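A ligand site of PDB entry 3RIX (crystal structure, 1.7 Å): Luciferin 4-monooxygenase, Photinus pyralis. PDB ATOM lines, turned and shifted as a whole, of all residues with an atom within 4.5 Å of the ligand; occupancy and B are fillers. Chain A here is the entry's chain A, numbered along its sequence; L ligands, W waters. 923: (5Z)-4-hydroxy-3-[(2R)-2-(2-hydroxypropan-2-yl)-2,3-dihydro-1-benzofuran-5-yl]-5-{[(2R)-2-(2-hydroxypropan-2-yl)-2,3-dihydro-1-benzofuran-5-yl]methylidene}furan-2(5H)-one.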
ATOM      1  N   ARG A 218      -7.558  -9.774  20.848  1.00  0.00           N
ATOM      2  CA  ARG A 218      -8.906 -10.295  20.726  1.00  0.00           C
ATOM      3  C   ARG A 218      -8.974 -11.418  19.711  1.00  0.00           C
ATOM      4  O   ARG A 218      -9.660 -12.416  19.924  1.00  0.00           O
ATOM      5  CB  ARG A 218      -9.877  -9.174  20.333  1.00  0.00           C
ATOM      6  CG  ARG A 218     -11.277  -9.686  19.927  1.00  0.00           C
ATOM      7  CD  ARG A 218     -12.119 -10.154  21.170  1.00  0.00           C
ATOM      8  NE  ARG A 218     -13.159 -11.070  20.708  1.00  0.00           N
ATOM      9  CZ  ARG A 218     -13.533 -12.183  21.322  1.00  0.00           C
ATOM     10  NH1 ARG A 218     -12.980 -12.517  22.500  1.00  0.00           N
ATOM     11  NH2 ARG A 218     -14.475 -12.947  20.795  1.00  0.00           N
ATOM     12  N   ALA A 222     -10.455 -15.175  20.099  1.00  0.00           N
ATOM     13  CA  ALA A 222     -11.690 -15.528  19.402  1.00  0.00           C
ATOM     14  C   ALA A 222     -11.661 -16.934  18.812  1.00  0.00           C
ATOM     15  O   ALA A 222     -12.696 -17.610  18.736  1.00  0.00           O
ATOM     16  CB  ALA A 222     -12.004 -14.472  18.273  1.00  0.00           C
ATOM     17  N   PHE A 227     -10.796 -20.437  25.058  1.00  0.00           N
ATOM     18  CA  PHE A 227     -11.336 -19.128  25.400  1.00  0.00           C
ATOM     19  C   PHE A 227     -12.181 -18.503  24.285  1.00  0.00           C
ATOM     20  O   PHE A 227     -12.687 -17.387  24.444  1.00  0.00           O
ATOM     21  CB  PHE A 227     -10.211 -18.199  25.805  1.00  0.00           C
ATOM     22  CG  PHE A 227      -9.628 -18.568  27.124  1.00  0.00           C
ATOM     23  CD1 PHE A 227      -8.538 -19.417  27.206  1.00  0.00           C
ATOM     24  CD2 PHE A 227     -10.209 -18.103  28.296  1.00  0.00           C
ATOM     25  CE1 PHE A 227      -8.024 -19.783  28.446  1.00  0.00           C
ATOM     26  CE2 PHE A 227      -9.698 -18.466  29.523  1.00  0.00           C
ATOM     27  CZ  PHE A 227      -8.604 -19.311  29.597  1.00  0.00           C
ATOM     28  N   GLY A 228     -12.326 -19.219  23.192  1.00  0.00           N
ATOM     29  CA  GLY A 228     -13.138 -18.759  22.075  1.00  0.00           C
ATOM     30  C   GLY A 228     -13.881 -19.901  21.421  1.00  0.00           C
ATOM     31  O   GLY A 228     -14.387 -20.794  22.106  1.00  0.00           O
ATOM     32  N   ASN A 229     -13.977 -19.866  20.096  1.00  0.00           N
ATOM     33  CA  ASN A 229     -14.610 -20.939  19.339  1.00  0.00           C
ATOM     34  C   ASN A 229     -13.584 -21.601  18.439  1.00  0.00           C
ATOM     35  O   ASN A 229     -12.857 -20.947  17.698  1.00  0.00           O
ATOM     36  CB  ASN A 229     -15.746 -20.414  18.443  1.00  0.00           C
ATOM     37  CG  ASN A 229     -16.862 -19.795  19.214  1.00  0.00           C
ATOM     38  OD1 ASN A 229     -17.152 -18.611  19.040  1.00  0.00           O
ATOM     39  ND2 ASN A 229     -17.521 -20.574  20.072  1.00  0.00           N
ATOM     40  N   HIS A 245     -21.141  -1.347  19.692  1.00  0.00           N
ATOM     41  CA  HIS A 245     -20.756  -1.586  21.087  1.00  0.00           C
ATOM     42  C   HIS A 245     -19.666  -2.653  21.131  1.00  0.00           C
ATOM     43  O   HIS A 245     -19.573  -3.509  20.265  1.00  0.00           O
ATOM     44  CB  HIS A 245     -22.006  -1.987  21.884  1.00  0.00           C
ATOM     45  CG  HIS A 245     -21.751  -2.397  23.302  1.00  0.00           C
ATOM     46  ND1 HIS A 245     -21.349  -3.676  23.649  1.00  0.00           N
ATOM     47  CD2 HIS A 245     -21.854  -1.705  24.462  1.00  0.00           C
ATOM     48  CE1 HIS A 245     -21.208  -3.750  24.968  1.00  0.00           C
ATOM     49  NE2 HIS A 245     -21.512  -2.562  25.481  1.00  0.00           N
ATOM     50  N   GLY A 246     -18.794  -2.617  22.134  1.00  0.00           N
ATOM     51  CA  GLY A 246     -17.661  -3.521  22.123  1.00  0.00           C
ATOM     52  C   GLY A 246     -18.004  -5.004  22.010  1.00  0.00           C
ATOM     53  O   GLY A 246     -17.291  -5.760  21.357  1.00  0.00           O
ATOM     54  N   PHE A 247     -19.085  -5.455  22.652  1.00  0.00           N
ATOM     55  CA  PHE A 247     -19.455  -6.858  22.603  1.00  0.00           C
ATOM     56  C   PHE A 247     -19.782  -7.220  21.147  1.00  0.00           C
ATOM     57  O   PHE A 247     -19.276  -8.218  20.626  1.00  0.00           O
ATOM     58  CB  PHE A 247     -20.659  -7.109  23.558  1.00  0.00           C
ATOM     59  CG  PHE A 247     -21.113  -8.544  23.658  1.00  0.00           C
ATOM     60  CD1 PHE A 247     -20.220  -9.605  23.688  1.00  0.00           C
ATOM     61  CD2 PHE A 247     -22.476  -8.834  23.828  1.00  0.00           C
ATOM     62  CE1 PHE A 247     -20.660 -10.926  23.857  1.00  0.00           C
ATOM     63  CE2 PHE A 247     -22.926 -10.140  23.973  1.00  0.00           C
ATOM     64  CZ  PHE A 247     -22.032 -11.194  23.982  1.00  0.00           C
ATOM     65  N   THR A 251     -16.817  -9.388  19.003  1.00  0.00           N
ATOM     66  CA  THR A 251     -17.224 -10.735  18.639  1.00  0.00           C
ATOM     67  C   THR A 251     -17.304 -10.851  17.117  1.00  0.00           C
ATOM     68  O   THR A 251     -16.878 -11.838  16.552  1.00  0.00           O
ATOM     69  CB  THR A 251     -18.565 -11.155  19.267  1.00  0.00           C
ATOM     70  OG1 THR A 251     -19.592 -10.204  18.931  1.00  0.00           O
ATOM     71  CG2 THR A 251     -18.423 -11.249  20.820  1.00  0.00           C
ATOM     72  N   TYR A 255     -15.407 -13.322  14.595  1.00  0.00           N
ATOM     73  CA  TYR A 255     -16.069 -14.313  13.761  1.00  0.00           C
ATOM     74  C   TYR A 255     -15.580 -14.258  12.317  1.00  0.00           C
ATOM     75  O   TYR A 255     -15.508 -15.286  11.656  1.00  0.00           O
ATOM     76  CB  TYR A 255     -17.582 -14.105  13.803  1.00  0.00           C
ATOM     77  CG  TYR A 255     -18.198 -14.349  15.160  1.00  0.00           C
ATOM     78  CD1 TYR A 255     -17.726 -15.333  15.987  1.00  0.00           C
ATOM     79  CD2 TYR A 255     -19.285 -13.578  15.593  1.00  0.00           C
ATOM     80  CE1 TYR A 255     -18.350 -15.581  17.248  1.00  0.00           C
ATOM     81  CE2 TYR A 255     -19.874 -13.786  16.831  1.00  0.00           C
ATOM     82  CZ  TYR A 255     -19.412 -14.790  17.641  1.00  0.00           C
ATOM     83  OH  TYR A 255     -20.023 -15.010  18.860  1.00  0.00           O
ATOM     84  N   GLU A 311     -24.287 -23.210  22.216  1.00  0.00           N
ATOM     85  CA  GLU A 311     -24.011 -22.281  23.295  1.00  0.00           C
ATOM     86  C   GLU A 311     -24.767 -20.977  23.129  1.00  0.00           C
ATOM     87  O   GLU A 311     -25.168 -20.607  22.025  1.00  0.00           O
ATOM     88  CB  GLU A 311     -22.500 -21.967  23.370  1.00  0.00           C
ATOM     89  CG  GLU A 311     -22.034 -21.018  22.303  1.00  0.00           C
ATOM     90  CD  GLU A 311     -20.531 -20.698  22.351  1.00  0.00           C
ATOM     91  OE1 GLU A 311     -19.813 -21.185  23.254  1.00  0.00           O
ATOM     92  OE2 GLU A 311     -20.092 -19.937  21.464  1.00  0.00           O
ATOM     93  N   ALA A 313     -24.004 -17.037  24.542  1.00  0.00           N
ATOM     94  CA  ALA A 313     -23.050 -16.186  25.252  1.00  0.00           C
ATOM     95  C   ALA A 313     -23.774 -14.937  25.732  1.00  0.00           C
ATOM     96  O   ALA A 313     -24.615 -14.399  25.024  1.00  0.00           O
ATOM     97  CB  ALA A 313     -21.912 -15.804  24.338  1.00  0.00           C
ATOM     98  N   SER A 314     -23.423 -14.458  26.917  1.00  0.00           N
ATOM     99  CA  SER A 314     -24.065 -13.248  27.427  1.00  0.00           C
ATOM    100  C   SER A 314     -23.001 -12.234  27.711  1.00  0.00           C
ATOM    101  O   SER A 314     -22.015 -12.554  28.365  1.00  0.00           O
ATOM    102  CB  SER A 314     -24.808 -13.521  28.743  1.00  0.00           C
ATOM    103  OG  SER A 314     -25.480 -12.328  29.174  1.00  0.00           O
ATOM    104  N   GLY A 315     -23.204 -11.019  27.221  1.00  0.00           N
ATOM    105  CA  GLY A 315     -22.267  -9.941  27.486  1.00  0.00           C
ATOM    106  C   GLY A 315     -22.961  -8.602  27.582  1.00  0.00           C
ATOM    107  O   GLY A 315     -24.144  -8.492  27.275  1.00  0.00           O
ATOM    108  N   GLY A 316     -22.230  -7.575  28.002  1.00  0.00           N
ATOM    109  CA  GLY A 316     -22.741  -6.231  28.059  1.00  0.00           C
ATOM    110  C   GLY A 316     -22.902  -5.731  29.481  1.00  0.00           C
ATOM    111  O   GLY A 316     -22.920  -4.529  29.727  1.00  0.00           O
ATOM    112  N   ALA A 317     -23.008  -6.654  30.422  1.00  0.00           N
ATOM    113  CA  ALA A 317     -23.230  -6.338  31.839  1.00  0.00           C
ATOM    114  C   ALA A 317     -23.395  -7.664  32.572  1.00  0.00           C
ATOM    115  O   ALA A 317     -23.950  -8.590  32.017  1.00  0.00           O
ATOM    116  CB  ALA A 317     -24.479  -5.486  31.995  1.00  0.00           C
ATOM    117  N   ARG A 337     -22.359 -19.414  28.337  1.00  0.00           N
ATOM    118  CA  ARG A 337     -20.987 -19.005  28.081  1.00  0.00           C
ATOM    119  C   ARG A 337     -20.887 -17.541  28.486  1.00  0.00           C
ATOM    120  O   ARG A 337     -21.284 -16.672  27.748  1.00  0.00           O
ATOM    121  CB  ARG A 337     -20.633 -19.194  26.608  1.00  0.00           C
ATOM    122  CG  ARG A 337     -19.149 -18.969  26.286  1.00  0.00           C
ATOM    123  CD  ARG A 337     -18.469 -20.294  26.136  1.00  0.00           C
ATOM    124  NE  ARG A 337     -17.003 -20.211  26.063  1.00  0.00           N
ATOM    125  CZ  ARG A 337     -16.298 -20.420  24.972  1.00  0.00           C
ATOM    126  NH1 ARG A 337     -16.890 -20.721  23.811  1.00  0.00           N
ATOM    127  NH2 ARG A 337     -14.961 -20.358  25.040  1.00  0.00           N
ATOM    128  N   GLN A 338     -20.404 -17.278  29.690  1.00  0.00           N
ATOM    129  CA  GLN A 338     -20.384 -15.917  30.196  1.00  0.00           C
ATOM    130  C   GLN A 338     -19.026 -15.288  29.996  1.00  0.00           C
ATOM    131  O   GLN A 338     -18.056 -15.961  29.686  1.00  0.00           O
ATOM    132  CB  GLN A 338     -20.710 -15.914  31.694  1.00  0.00           C
ATOM    133  CG  GLN A 338     -22.055 -16.523  32.015  1.00  0.00           C
ATOM    134  CD  GLN A 338     -22.498 -16.226  33.440  1.00  0.00           C
ATOM    135  OE1 GLN A 338     -22.899 -17.127  34.187  1.00  0.00           O
ATOM    136  NE2 GLN A 338     -22.426 -14.954  33.830  1.00  0.00           N
ATOM    137  N   GLY A 339     -18.979 -13.979  30.146  1.00  0.00           N
ATOM    138  CA  GLY A 339     -17.720 -13.273  30.118  1.00  0.00           C
ATOM    139  C   GLY A 339     -17.900 -11.916  30.743  1.00  0.00           C
ATOM    140  O   GLY A 339     -19.027 -11.475  30.965  1.00  0.00           O
ATOM    141  N   TYR A 340     -16.795 -11.245  31.040  1.00  0.00           N
ATOM    142  CA  TYR A 340     -16.851  -9.925  31.632  1.00  0.00           C
ATOM    143  C   TYR A 340     -15.895  -9.025  30.904  1.00  0.00           C
ATOM    144  O   TYR A 340     -14.732  -9.376  30.777  1.00  0.00           O
ATOM    145  CB  TYR A 340     -16.443  -9.979  33.125  1.00  0.00           C
ATOM    146  CG  TYR A 340     -16.406  -8.623  33.768  1.00  0.00           C
ATOM    147  CD1 TYR A 340     -15.242  -7.851  33.781  1.00  0.00           C
ATOM    148  CD2 TYR A 340     -17.537  -8.107  34.399  1.00  0.00           C
ATOM    149  CE1 TYR A 340     -15.218  -6.604  34.371  1.00  0.00           C
ATOM    150  CE2 TYR A 340     -17.506  -6.866  35.016  1.00  0.00           C
ATOM    151  CZ  TYR A 340     -16.342  -6.128  34.998  1.00  0.00           C
ATOM    152  OH  TYR A 340     -16.306  -4.889  35.592  1.00  0.00           O
ATOM    153  N   GLY A 341     -16.394  -7.903  30.402  1.00  0.00           N
ATOM    154  CA  GLY A 341     -15.552  -6.891  29.791  1.00  0.00           C
ATOM    155  C   GLY A 341     -16.101  -5.501  30.042  1.00  0.00           C
ATOM    156  O   GLY A 341     -17.171  -5.333  30.656  1.00  0.00           O
ATOM    157  N   LEU A 342     -15.346  -4.512  29.584  1.00  0.00           N
ATOM    158  CA  LEU A 342     -15.737  -3.131  29.618  1.00  0.00           C
ATOM    159  C   LEU A 342     -15.284  -2.529  28.284  1.00  0.00           C
ATOM    160  O   LEU A 342     -14.408  -3.081  27.607  1.00  0.00           O
ATOM    161  CB  LEU A 342     -14.983  -2.383  30.716  1.00  0.00           C
ATOM    162  CG  LEU A 342     -15.167  -2.968  32.133  1.00  0.00           C
ATOM    163  CD1 LEU A 342     -14.132  -2.390  33.056  1.00  0.00           C
ATOM    164  CD2 LEU A 342     -16.580  -2.668  32.606  1.00  0.00           C
ATOM    165  N   THR A 343     -15.850  -1.389  27.932  1.00  0.00           N
ATOM    166  CA  THR A 343     -15.441  -0.738  26.673  1.00  0.00           C
ATOM    167  C   THR A 343     -13.938  -0.476  26.768  1.00  0.00           C
ATOM    168  O   THR A 343     -13.175  -0.698  25.809  1.00  0.00           O
ATOM    169  CB  THR A 343     -16.221   0.541  26.493  1.00  0.00           C
ATOM    170  OG1 THR A 343     -17.619   0.208  26.452  1.00  0.00           O
ATOM    171  CG2 THR A 343     -15.817   1.270  25.157  1.00  0.00           C
ATOM    172  N   THR A 346     -11.509  -3.282  25.745  1.00  0.00           N
ATOM    173  CA  THR A 346     -11.789  -3.746  24.381  1.00  0.00           C
ATOM    174  C   THR A 346     -12.957  -4.735  24.355  1.00  0.00           C
ATOM    175  O   THR A 346     -13.996  -4.430  23.763  1.00  0.00           O
ATOM    176  CB  THR A 346     -10.556  -4.369  23.705  1.00  0.00           C
ATOM    177  OG1 THR A 346      -9.486  -3.407  23.682  1.00  0.00           O
ATOM    178  CG2 THR A 346     -10.892  -4.767  22.251  1.00  0.00           C
ATOM    179  N   SER A 347     -12.805  -5.885  25.001  1.00  0.00           N
ATOM    180  CA  SER A 347     -13.856  -6.924  25.008  1.00  0.00           C
ATOM    181  C   SER A 347     -13.710  -7.704  26.307  1.00  0.00           C
ATOM    182  O   SER A 347     -13.190  -7.180  27.285  1.00  0.00           O
ATOM    183  CB  SER A 347     -13.686  -7.853  23.804  1.00  0.00           C
ATOM    184  OG  SER A 347     -14.802  -8.716  23.644  1.00  0.00           O
ATOM    185  N   ALA A 348     -14.164  -8.958  26.323  1.00  0.00           N
ATOM    186  CA  ALA A 348     -14.123  -9.725  27.577  1.00  0.00           C
ATOM    187  C   ALA A 348     -12.681 -10.093  27.921  1.00  0.00           C
ATOM    188  O   ALA A 348     -11.950 -10.603  27.074  1.00  0.00           O
ATOM    189  CB  ALA A 348     -14.953 -10.979  27.452  1.00  0.00           C
ATOM    190  N   ILE A 351     -13.465 -14.941  30.514  1.00  0.00           N
ATOM    191  CA  ILE A 351     -14.354 -15.718  29.640  1.00  0.00           C
ATOM    192  C   ILE A 351     -14.519 -17.133  30.171  1.00  0.00           C
ATOM    193  O   ILE A 351     -13.547 -17.772  30.574  1.00  0.00           O
ATOM    194  CB  ILE A 351     -13.809 -15.803  28.208  1.00  0.00           C
ATOM    195  CG1 ILE A 351     -13.686 -14.405  27.616  1.00  0.00           C
ATOM    196  CG2 ILE A 351     -14.709 -16.729  27.339  1.00  0.00           C
ATOM    197  CD1 ILE A 351     -12.971 -14.345  26.249  1.00  0.00           C
HETATM  198  C1  923 L   1     -17.484 -12.186  25.437  1.00  0.00           C
HETATM  199  C2  923 L   1     -18.426 -12.124  26.473  1.00  0.00           C
HETATM  200  C3  923 L   1     -19.153 -13.257  26.860  1.00  0.00           C
HETATM  201  C4  923 L   1     -18.895 -14.486  26.259  1.00  0.00           C
HETATM  202  C5  923 L   1     -17.918 -14.554  25.280  1.00  0.00           C
HETATM  203  C6  923 L   1     -17.242 -13.434  24.881  1.00  0.00           C
HETATM  204  C7  923 L   1     -16.265 -13.796  23.787  1.00  0.00           C
HETATM  205  C8  923 L   1     -16.428 -15.320  23.775  1.00  0.00           C
HETATM  206  O9  923 L   1     -17.544 -15.693  24.618  1.00  0.00           O
HETATM  207  C10 923 L   1     -18.810 -10.873  27.150  1.00  0.00           C
HETATM  208  C11 923 L   1     -18.417  -9.533  26.705  1.00  0.00           C
HETATM  209  O12 923 L   1     -17.717  -9.204  25.714  1.00  0.00           O
HETATM  210  C13 923 L   1     -17.643  -7.926  25.683  1.00  0.00           C
HETATM  211  C14 923 L   1     -18.342  -7.306  26.735  1.00  0.00           C
HETATM  212  C15 923 L   1     -18.828  -8.419  27.371  1.00  0.00           C
HETATM  213  C16 923 L   1     -18.512  -5.871  27.062  1.00  0.00           C
HETATM  214  C17 923 L   1     -19.181  -5.478  28.232  1.00  0.00           C
HETATM  215  C18 923 L   1     -19.306  -4.121  28.468  1.00  0.00           C
HETATM  216  C19 923 L   1     -18.835  -3.172  27.610  1.00  0.00           C
HETATM  217  C20 923 L   1     -18.183  -3.538  26.443  1.00  0.00           C
HETATM  218  C21 923 L   1     -18.025  -4.897  26.175  1.00  0.00           C
HETATM  219  C22 923 L   1     -19.966  -3.406  29.607  1.00  0.00           C
HETATM  220  C23 923 L   1     -19.884  -1.924  29.226  1.00  0.00           C
HETATM  221  O24 923 L   1     -19.088  -1.888  28.012  1.00  0.00           O
HETATM  222  C25 923 L   1     -21.246  -1.280  29.025  1.00  0.00           C
HETATM  223  C26 923 L   1     -21.944  -1.116  30.366  1.00  0.00           C
HETATM  224  O27 923 L   1     -22.062  -2.125  28.198  1.00  0.00           O
HETATM  225  C28 923 L   1     -21.089   0.090  28.387  1.00  0.00           C
HETATM  226  C29 923 L   1     -16.679 -15.874  22.381  1.00  0.00           C
HETATM  227  O30 923 L   1     -15.548 -15.599  21.548  1.00  0.00           O
HETATM  228  C31 923 L   1     -17.959 -15.242  21.825  1.00  0.00           C
HETATM  229  C32 923 L   1     -16.822 -17.390  22.463  1.00  0.00           C
HETATM  230  O33 923 L   1     -16.987  -7.299  24.782  1.00  0.00           O
HETATM  231  O34 923 L   1     -19.694  -8.425  28.558  1.00  0.00           O
HETATM  232  O   HOH W   1     -13.069 -15.356  22.680  1.00  0.00           O
HETATM  233  O   HOH W   2     -15.403 -16.617  19.062  1.00  0.00           O
HETATM  234  O   HOH W   3     -17.474   0.643  29.774  1.00  0.00           O
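The backbone NH (N) of Gly 316 sits at hydrogen-bond distance from an oxygen (O34) of the ligand (2.7 Å). O of Gly 316 is in hydrogen-bond range of O27 of the ligand (3.0 Å). The side-chain hydroxyl of Ser 347 lies within hydrogen-bond range of an oxygen (O33) of the ligand, at 2.8 Å. An oxygen (O30) of the ligand lies within hydrogen-bond range of the guanidinium group (NH2) of Arg 218, at 3.0 Å. A ring nitrogen (NE2) of His 245 is in hydrogen-bond range of an oxygen (O27) of the ligand (2.8 Å). The side-chain hydroxyl (OG1) of Thr 343 sits at hydrogen-bond distance from an oxygen (O24) of the ligand. An oxygen (O24) of the ligand sits at hydrogen-bond distance from the backbone NH (N) of Thr 343 (3.3 Å).
The guanidinium group (NH2) of Arg 337 sits at hydrogen-bond distance from the backbone carbonyl oxygen (O) of Gly 228. The backbone carbonyl oxygen (O) of Ala 222 is in hydrogen-bond range of the backbone NH (N) of Asn 229 (2.9 Å). OE1 of Glu 311 lies within salt-bridge range of NH1 of Arg 337 (3.0 Å). OE2 of Glu 311 sits at hydrogen-bond distance from ND2 of Asn 229, 3.0 Å away. The backbone NH (N) of Phe 247 lies within hydrogen-bond range of a ring nitrogen (ND1) of His 245, 3.0 Å away. OG1 of Thr 251 lies within hydrogen-bond range of O of Phe 247 (2.6 Å). O of Arg 337 sits at hydrogen-bond distance from N of Ser 314, at 3.2 Å.
Gly 228 touches the ligand (CA to C32, 3.9 Å). OD1 of Asn 229 touches C32 of the ligand (3.6 Å). Gly 246 touches the ligand (C to O33, 3.7 Å). Phe 247 touches the ligand (CD1 to O12, 3.2 Å). Tyr 255 touches the ligand (OH to C31, 3.6 Å). CB of Ala 313 touches C4 of the ligand, 3.8 Å away. O of Ser 314 touches C3 of the ligand, 3.3 Å away. Gly 315 touches the ligand. Arg 337 touches the ligand (O to C4, 3.6 Å). Gln 338 touches the ligand. Gly 339 touches the ligand. O of Gly 341 touches C17 of the ligand (3.2 Å). C of Leu 342 touches C20 of the ligand (3.6 Å). Ala 348 touches the ligand (CB to C1, 3.5 Å). Hydrophobic or aromatic side chains that line the ligand: His 245, Phe 247, Ala 313 and Ala 348. The nearest printed residue that does not touch the ligand is Ile 351 (4.1 Å).
Water W2 lies within hydrogen-bond range of OD1 of Asn 229 (2.7 Å), O30 of the ligand (2.7 Å) and O of Ala 222 (2.9 Å). Water W1 lies within hydrogen-bond range of O of Phe 227, O30 of the ligand and NH1 of Arg 218. Water W3 bridges N of Thr 343 and O24 of the ligand.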
